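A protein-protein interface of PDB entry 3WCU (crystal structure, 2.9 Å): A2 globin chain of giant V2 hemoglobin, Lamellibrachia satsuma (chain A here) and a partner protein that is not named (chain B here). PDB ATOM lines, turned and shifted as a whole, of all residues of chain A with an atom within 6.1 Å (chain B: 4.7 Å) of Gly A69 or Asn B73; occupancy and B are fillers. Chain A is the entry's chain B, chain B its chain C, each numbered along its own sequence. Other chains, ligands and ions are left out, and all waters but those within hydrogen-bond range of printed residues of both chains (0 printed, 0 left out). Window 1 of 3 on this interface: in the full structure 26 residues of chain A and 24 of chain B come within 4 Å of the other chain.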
ATOM      1  N   TRP A  15       4.122 -22.429  23.480  1.00  0.00           N
ATOM      2  CA  TRP A  15       2.995 -22.456  22.552  1.00  0.00           C
ATOM      3  C   TRP A  15       1.872 -21.622  23.083  1.00  0.00           C
ATOM      4  O   TRP A  15       1.436 -20.686  22.427  1.00  0.00           O
ATOM      5  CB  TRP A  15       2.494 -23.893  22.329  1.00  0.00           C
ATOM      6  CG  TRP A  15       1.110 -23.975  21.737  1.00  0.00           C
ATOM      7  CD1 TRP A  15      -0.058 -24.183  22.415  1.00  0.00           C
ATOM      8  CD2 TRP A  15       0.756 -23.826  20.363  1.00  0.00           C
ATOM      9  NE1 TRP A  15      -1.120 -24.175  21.545  1.00  0.00           N
ATOM     10  CE2 TRP A  15      -0.647 -23.957  20.276  1.00  0.00           C
ATOM     11  CE3 TRP A  15       1.485 -23.593  19.193  1.00  0.00           C
ATOM     12  CZ2 TRP A  15      -1.335 -23.865  19.064  1.00  0.00           C
ATOM     13  CZ3 TRP A  15       0.802 -23.499  17.988  1.00  0.00           C
ATOM     14  CH2 TRP A  15      -0.595 -23.636  17.935  1.00  0.00           C
ATOM     15  N   TYR A  19       0.271 -18.840  21.134  1.00  0.00           N
ATOM     16  CA  TYR A  19      -1.073 -19.087  20.611  1.00  0.00           C
ATOM     17  C   TYR A  19      -2.006 -18.040  21.176  1.00  0.00           C
ATOM     18  O   TYR A  19      -3.175 -17.949  20.803  1.00  0.00           O
ATOM     19  CB  TYR A  19      -1.542 -20.494  21.004  1.00  0.00           C
ATOM     20  CG  TYR A  19      -2.921 -20.890  20.505  1.00  0.00           C
ATOM     21  CD1 TYR A  19      -3.398 -20.461  19.266  1.00  0.00           C
ATOM     22  CD2 TYR A  19      -3.728 -21.742  21.258  1.00  0.00           C
ATOM     23  CE1 TYR A  19      -4.650 -20.874  18.791  1.00  0.00           C
ATOM     24  CE2 TYR A  19      -4.973 -22.165  20.794  1.00  0.00           C
ATOM     25  CZ  TYR A  19      -5.431 -21.730  19.563  1.00  0.00           C
ATOM     26  OH  TYR A  19      -6.669 -22.158  19.123  1.00  0.00           O
ATOM     27  N   ALA A  64      -8.339 -22.269   9.569  1.00  0.00           N
ATOM     28  CA  ALA A  64      -7.077 -22.167  10.307  1.00  0.00           C
ATOM     29  C   ALA A  64      -7.356 -22.179  11.808  1.00  0.00           C
ATOM     30  O   ALA A  64      -6.569 -22.721  12.586  1.00  0.00           O
ATOM     31  CB  ALA A  64      -6.319 -20.888   9.920  1.00  0.00           C
ATOM     32  N   THR A  65      -8.470 -21.572  12.213  1.00  0.00           N
ATOM     33  CA  THR A  65      -8.825 -21.572  13.625  1.00  0.00           C
ATOM     34  C   THR A  65      -9.034 -23.041  14.024  1.00  0.00           C
ATOM     35  O   THR A  65      -8.571 -23.476  15.085  1.00  0.00           O
ATOM     36  CB  THR A  65     -10.122 -20.730  13.905  1.00  0.00           C
ATOM     37  OG1 THR A  65      -9.843 -19.337  13.731  1.00  0.00           O
ATOM     38  CG2 THR A  65     -10.617 -20.945  15.331  1.00  0.00           C
ATOM     39  N   ARG A  66      -9.704 -23.807  13.154  1.00  0.00           N
ATOM     40  CA  ARG A  66      -9.973 -25.235  13.392  1.00  0.00           C
ATOM     41  C   ARG A  66      -8.682 -26.059  13.453  1.00  0.00           C
ATOM     42  O   ARG A  66      -8.536 -26.943  14.307  1.00  0.00           O
ATOM     43  CB  ARG A  66     -10.899 -25.781  12.298  1.00  0.00           C
ATOM     44  CG  ARG A  66     -12.293 -26.197  12.781  1.00  0.00           C
ATOM     45  CD  ARG A  66     -13.345 -25.822  11.746  1.00  0.00           C
ATOM     46  NE  ARG A  66     -12.846 -26.045  10.394  1.00  0.00           N
ATOM     47  CZ  ARG A  66     -13.133 -25.276   9.348  1.00  0.00           C
ATOM     48  NH1 ARG A  66     -12.619 -25.565   8.157  1.00  0.00           N
ATOM     49  NH2 ARG A  66     -13.925 -24.218   9.492  1.00  0.00           N
ATOM     50  N   VAL A  67      -7.748 -25.760  12.552  1.00  0.00           N
ATOM     51  CA  VAL A  67      -6.463 -26.459  12.528  1.00  0.00           C
ATOM     52  C   VAL A  67      -5.649 -26.174  13.792  1.00  0.00           C
ATOM     53  O   VAL A  67      -5.441 -27.076  14.614  1.00  0.00           O
ATOM     54  CB  VAL A  67      -5.598 -26.050  11.304  1.00  0.00           C
ATOM     55  CG1 VAL A  67      -4.208 -26.652  11.423  1.00  0.00           C
ATOM     56  CG2 VAL A  67      -6.262 -26.508  10.014  1.00  0.00           C
ATOM     57  N   LEU A  68      -5.191 -24.923  13.934  1.00  0.00           N
ATOM     58  CA  LEU A  68      -4.389 -24.501  15.084  1.00  0.00           C
ATOM     59  C   LEU A  68      -5.108 -24.842  16.378  1.00  0.00           C
ATOM     60  O   LEU A  68      -4.473 -25.079  17.405  1.00  0.00           O
ATOM     61  CB  LEU A  68      -4.096 -22.999  15.025  1.00  0.00           C
ATOM     62  CG  LEU A  68      -3.379 -22.452  13.782  1.00  0.00           C
ATOM     63  CD1 LEU A  68      -3.015 -20.983  14.028  1.00  0.00           C
ATOM     64  CD2 LEU A  68      -2.128 -23.268  13.476  1.00  0.00           C
ATOM     65  N   GLY A  69      -6.434 -24.868  16.319  1.00  0.00           N
ATOM     66  CA  GLY A  69      -7.211 -25.225  17.489  1.00  0.00           C
ATOM     67  C   GLY A  69      -6.921 -26.674  17.849  1.00  0.00           C
ATOM     68  O   GLY A  69      -6.925 -27.053  19.028  1.00  0.00           O
ATOM     69  N   GLY A  70      -6.677 -27.487  16.822  1.00  0.00           N
ATOM     70  CA  GLY A  70      -6.362 -28.884  17.043  1.00  0.00           C
ATOM     71  C   GLY A  70      -4.930 -29.052  17.527  1.00  0.00           C
ATOM     72  O   GLY A  70      -4.652 -29.820  18.458  1.00  0.00           O
ATOM     73  N   LEU A  71      -4.017 -28.320  16.894  1.00  0.00           N
ATOM     74  CA  LEU A  71      -2.610 -28.391  17.256  1.00  0.00           C
ATOM     75  C   LEU A  71      -2.521 -28.167  18.751  1.00  0.00           C
ATOM     76  O   LEU A  71      -1.691 -28.769  19.431  1.00  0.00           O
ATOM     77  CB  LEU A  71      -1.798 -27.315  16.517  1.00  0.00           C
ATOM     78  CG  LEU A  71      -0.373 -27.690  16.071  1.00  0.00           C
ATOM     79  CD1 LEU A  71       0.322 -26.457  15.479  1.00  0.00           C
ATOM     80  CD2 LEU A  71       0.428 -28.279  17.235  1.00  0.00           C
ATOM     81  N   ASP A  72      -3.393 -27.302  19.259  1.00  0.00           N
ATOM     82  CA  ASP A  72      -3.410 -27.004  20.678  1.00  0.00           C
ATOM     83  C   ASP A  72      -3.754 -28.281  21.422  1.00  0.00           C
ATOM     84  O   ASP A  72      -2.947 -28.769  22.217  1.00  0.00           O
ATOM     85  CB  ASP A  72      -4.448 -25.925  21.001  1.00  0.00           C
ATOM     86  CG  ASP A  72      -4.341 -25.418  22.433  1.00  0.00           C
ATOM     87  OD1 ASP A  72      -5.366 -24.983  22.992  1.00  0.00           O
ATOM     88  OD2 ASP A  72      -3.227 -25.446  22.993  1.00  0.00           O
ATOM     89  N   MET A  73      -4.951 -28.815  21.161  1.00  0.00           N
ATOM     90  CA  MET A  73      -5.427 -30.052  21.795  1.00  0.00           C
ATOM     91  C   MET A  73      -4.281 -31.015  22.052  1.00  0.00           C
ATOM     92  O   MET A  73      -4.146 -31.569  23.148  1.00  0.00           O
ATOM     93  CB  MET A  73      -6.465 -30.749  20.907  1.00  0.00           C
ATOM     94  CG  MET A  73      -7.916 -30.365  21.182  1.00  0.00           C
ATOM     95  SD  MET A  73      -8.680 -31.128  22.660  1.00  0.00           S
ATOM     96  CE  MET A  73      -7.259 -32.072  23.369  1.00  0.00           C
ATOM     97  N   CYS A  74      -3.458 -31.188  21.019  1.00  0.00           N
ATOM     98  CA  CYS A  74      -2.308 -32.077  21.061  1.00  0.00           C
ATOM     99  C   CYS A  74      -1.194 -31.604  21.983  1.00  0.00           C
ATOM    100  O   CYS A  74      -0.803 -32.333  22.905  1.00  0.00           O
ATOM    101  CB  CYS A  74      -1.754 -32.294  19.644  1.00  0.00           C
ATOM    102  SG  CYS A  74      -2.825 -33.267  18.544  1.00  0.00           S
ATOM    103  N   TRP B  21      -8.146 -21.364  31.202  1.00  0.00           N
ATOM    104  CA  TRP B  21      -7.946 -22.348  30.129  1.00  0.00           C
ATOM    105  C   TRP B  21      -6.792 -22.106  29.158  1.00  0.00           C
ATOM    106  O   TRP B  21      -6.901 -21.304  28.224  1.00  0.00           O
ATOM    107  CB  TRP B  21      -9.263 -22.499  29.349  1.00  0.00           C
ATOM    108  CG  TRP B  21      -9.265 -23.568  28.295  1.00  0.00           C
ATOM    109  CD1 TRP B  21      -8.774 -23.471  27.025  1.00  0.00           C
ATOM    110  CD2 TRP B  21      -9.793 -24.895  28.420  1.00  0.00           C
ATOM    111  NE1 TRP B  21      -8.964 -24.654  26.349  1.00  0.00           N
ATOM    112  CE2 TRP B  21      -9.588 -25.543  27.183  1.00  0.00           C
ATOM    113  CE3 TRP B  21     -10.416 -25.599  29.457  1.00  0.00           C
ATOM    114  CZ2 TRP B  21      -9.984 -26.858  26.958  1.00  0.00           C
ATOM    115  CZ3 TRP B  21     -10.807 -26.904  29.233  1.00  0.00           C
ATOM    116  CH2 TRP B  21     -10.589 -27.521  27.993  1.00  0.00           C
ATOM    117  N   ARG B  29      -7.301 -28.094  32.291  1.00  0.00           N
ATOM    118  CA  ARG B  29      -8.294 -28.342  31.259  1.00  0.00           C
ATOM    119  C   ARG B  29      -9.115 -29.584  31.584  1.00  0.00           C
ATOM    120  O   ARG B  29     -10.329 -29.501  31.753  1.00  0.00           O
ATOM    121  CB  ARG B  29      -7.599 -28.509  29.916  1.00  0.00           C
ATOM    122  CG  ARG B  29      -6.362 -27.656  29.792  1.00  0.00           C
ATOM    123  CD  ARG B  29      -5.808 -27.699  28.388  1.00  0.00           C
ATOM    124  NE  ARG B  29      -6.702 -27.044  27.442  1.00  0.00           N
ATOM    125  CZ  ARG B  29      -6.411 -26.824  26.165  1.00  0.00           C
ATOM    126  NH1 ARG B  29      -5.243 -27.208  25.669  1.00  0.00           N
ATOM    127  NH2 ARG B  29      -7.287 -26.207  25.382  1.00  0.00           N
ATOM    128  N   ILE B  69     -12.117 -32.725  26.449  1.00  0.00           N
ATOM    129  CA  ILE B  69     -11.188 -31.672  26.112  1.00  0.00           C
ATOM    130  C   ILE B  69     -11.509 -31.098  24.723  1.00  0.00           C
ATOM    131  O   ILE B  69     -11.481 -29.885  24.543  1.00  0.00           O
ATOM    132  CB  ILE B  69      -9.740 -32.201  26.209  1.00  0.00           C
ATOM    133  CG1 ILE B  69      -9.492 -32.693  27.642  1.00  0.00           C
ATOM    134  CG2 ILE B  69      -8.745 -31.099  25.888  1.00  0.00           C
ATOM    135  CD1 ILE B  69      -8.123 -33.292  27.884  1.00  0.00           C
ATOM    136  N   ARG B  70     -11.839 -31.949  23.752  1.00  0.00           N
ATOM    137  CA  ARG B  70     -12.190 -31.481  22.399  1.00  0.00           C
ATOM    138  C   ARG B  70     -13.401 -30.524  22.385  1.00  0.00           C
ATOM    139  O   ARG B  70     -13.358 -29.472  21.745  1.00  0.00           O
ATOM    140  CB  ARG B  70     -12.510 -32.662  21.458  1.00  0.00           C
ATOM    141  CG  ARG B  70     -11.317 -33.497  20.975  1.00  0.00           C
ATOM    142  CD  ARG B  70     -11.708 -34.424  19.807  1.00  0.00           C
ATOM    143  NE  ARG B  70     -12.857 -35.274  20.123  1.00  0.00           N
ATOM    144  CZ  ARG B  70     -12.798 -36.409  20.818  1.00  0.00           C
ATOM    145  NH1 ARG B  70     -11.638 -36.863  21.280  1.00  0.00           N
ATOM    146  NH2 ARG B  70     -13.913 -37.085  21.066  1.00  0.00           N
ATOM    147  N   VAL B  71     -14.480 -30.906  23.067  1.00  0.00           N
ATOM    148  CA  VAL B  71     -15.695 -30.094  23.119  1.00  0.00           C
ATOM    149  C   VAL B  71     -15.393 -28.732  23.724  1.00  0.00           C
ATOM    150  O   VAL B  71     -15.676 -27.708  23.100  1.00  0.00           O
ATOM    151  CB  VAL B  71     -16.821 -30.788  23.958  1.00  0.00           C
ATOM    152  CG1 VAL B  71     -18.023 -29.870  24.121  1.00  0.00           C
ATOM    153  CG2 VAL B  71     -17.264 -32.057  23.270  1.00  0.00           C
ATOM    154  N   VAL B  72     -14.822 -28.718  24.932  1.00  0.00           N
ATOM    155  CA  VAL B  72     -14.493 -27.464  25.605  1.00  0.00           C
ATOM    156  C   VAL B  72     -13.461 -26.682  24.799  1.00  0.00           C
ATOM    157  O   VAL B  72     -13.579 -25.462  24.661  1.00  0.00           O
ATOM    158  CB  VAL B  72     -13.988 -27.700  27.054  1.00  0.00           C
ATOM    159  CG1 VAL B  72     -13.533 -26.385  27.684  1.00  0.00           C
ATOM    160  CG2 VAL B  72     -15.111 -28.254  27.902  1.00  0.00           C
ATOM    161  N   ASN B  73     -12.455 -27.365  24.260  1.00  0.00           N
ATOM    162  CA  ASN B  73     -11.473 -26.674  23.434  1.00  0.00           C
ATOM    163  C   ASN B  73     -12.219 -26.089  22.219  1.00  0.00           C
ATOM    164  O   ASN B  73     -11.713 -25.207  21.522  1.00  0.00           O
ATOM    165  CB  ASN B  73     -10.377 -27.620  22.940  1.00  0.00           C
ATOM    166  CG  ASN B  73      -9.223 -26.876  22.278  1.00  0.00           C
ATOM    167  OD1 ASN B  73      -8.289 -26.432  22.949  1.00  0.00           O
ATOM    168  ND2 ASN B  73      -9.294 -26.719  20.955  1.00  0.00           N
ATOM    169  N   GLY B  74     -13.424 -26.592  21.965  1.00  0.00           N
ATOM    170  CA  GLY B  74     -14.211 -26.086  20.854  1.00  0.00           C
ATOM    171  C   GLY B  74     -14.765 -24.735  21.234  1.00  0.00           C
ATOM    172  O   GLY B  74     -14.766 -23.801  20.430  1.00  0.00           O
ATOM    173  N   LEU B  75     -15.230 -24.650  22.481  1.00  0.00           N
ATOM    174  CA  LEU B  75     -15.778 -23.431  23.060  1.00  0.00           C
ATOM    175  C   LEU B  75     -14.661 -22.411  23.097  1.00  0.00           C
ATOM    176  O   LEU B  75     -14.867 -21.236  22.810  1.00  0.00           O
ATOM    177  CB  LEU B  75     -16.249 -23.718  24.473  1.00  0.00           C
ATOM    178  CG  LEU B  75     -16.892 -22.621  25.326  1.00  0.00           C
ATOM    179  CD1 LEU B  75     -18.172 -22.118  24.669  1.00  0.00           C
ATOM    180  CD2 LEU B  75     -17.179 -23.186  26.734  1.00  0.00           C
ATOM    181  N   ASP B  76     -13.465 -22.868  23.452  1.00  0.00           N
ATOM    182  CA  ASP B  76     -12.315 -21.982  23.514  1.00  0.00           C
ATOM    183  C   ASP B  76     -12.128 -21.289  22.183  1.00  0.00           C
ATOM    184  O   ASP B  76     -12.077 -20.068  22.115  1.00  0.00           O
ATOM    185  CB  ASP B  76     -11.048 -22.768  23.877  1.00  0.00           C
ATOM    186  CG  ASP B  76      -9.772 -21.932  23.751  1.00  0.00           C
ATOM    187  OD1 ASP B  76      -8.891 -22.053  24.624  1.00  0.00           O
ATOM    188  OD2 ASP B  76      -9.637 -21.166  22.776  1.00  0.00           O
ATOM    189  N   SER B  77     -12.028 -22.074  21.123  1.00  0.00           N
ATOM    190  CA  SER B  77     -11.837 -21.515  19.807  1.00  0.00           C
ATOM    191  C   SER B  77     -12.888 -20.458  19.540  1.00  0.00           C
ATOM    192  O   SER B  77     -12.580 -19.395  18.999  1.00  0.00           O
ATOM    193  CB  SER B  77     -11.927 -22.618  18.769  1.00  0.00           C
ATOM    194  OG  SER B  77     -10.985 -23.632  19.061  1.00  0.00           O
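The guanidinium group of Arg B29 lies within salt-bridge range of the side-chain carboxylate of Asp A72, 3.3 Å away. O of Gly A69 sits at hydrogen-bond distance from ND2 of Asn B73, 3.1 Å away. The side-chain sulfur of Met A73 lies close to the backbone carbonyl oxygen of Ile B69 (3.6 Å). The side-chain amide oxygen of Asn B73 lies close to the side-chain carboxylate of Asp A72 (3.3 Å). The side-chain sulfur of Met A73 lies within hydrogen-bond range of the backbone NH of Arg B70 (3.4 Å).
The side-chain carboxylate (OD2) of Asp A72 lies within hydrogen-bond range of the indole nitrogen (NE1) of Trp A15, 2.9 Å away. The side-chain hydroxyl (OG) of Ser B77 is in hydrogen-bond range of the backbone carbonyl oxygen (O) of Asn B73, 3.0 Å away. The side-chain amide oxygen (OD1) of Asn B73 lies within hydrogen-bond range of the guanidinium group (NH2) of Arg B29. The guanidinium group (NH2) of Arg B29 lies close to the indole nitrogen (NE1) of Trp B21.
Hydrophobic or aromatic side chains of chain B within 4 Å of the printed part of chain A: Ile B69. Of the 13 printed residues of chain A, 3 touch a printed residue of chain B. Hydrophobic or aromatic side chains of chain A that line the printed part of chain B: Met A73. Among the printed residues, Asp or Glu carboxylates within 4 Å of a Lys or Arg side-chain nitrogen of the other chain: Asp A72 with Arg B29 (3.3 Å).
Gly A69 touches one residue of chain B. Of the printed residues of chain B, Asp A72 touches Arg B29 and Asn B73. Of the printed residues of chain B, Met A73 touches Ile B69 (3.1 Å), Arg B70 (3.4 Å) and Asn B73 (3.9 Å). Trp B21 touches none of the printed residues of chain A. Of the printed residues of chain A, Arg B29 touches Asp A72. Of the printed residues of chain A, Ile B69 touches Met A73. Asn B73 touches three residues of chain A. The nearest residue of chain B that does not touch Gly A69 is Ser B77 (4.4 Å). The nearest residue of chain A that does not touch Asn B73 is Gly A70 (5.0 Å).
Among the printed residues, merely in contact across the chains: Met A73 with Asn B73 (3.9 Å).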
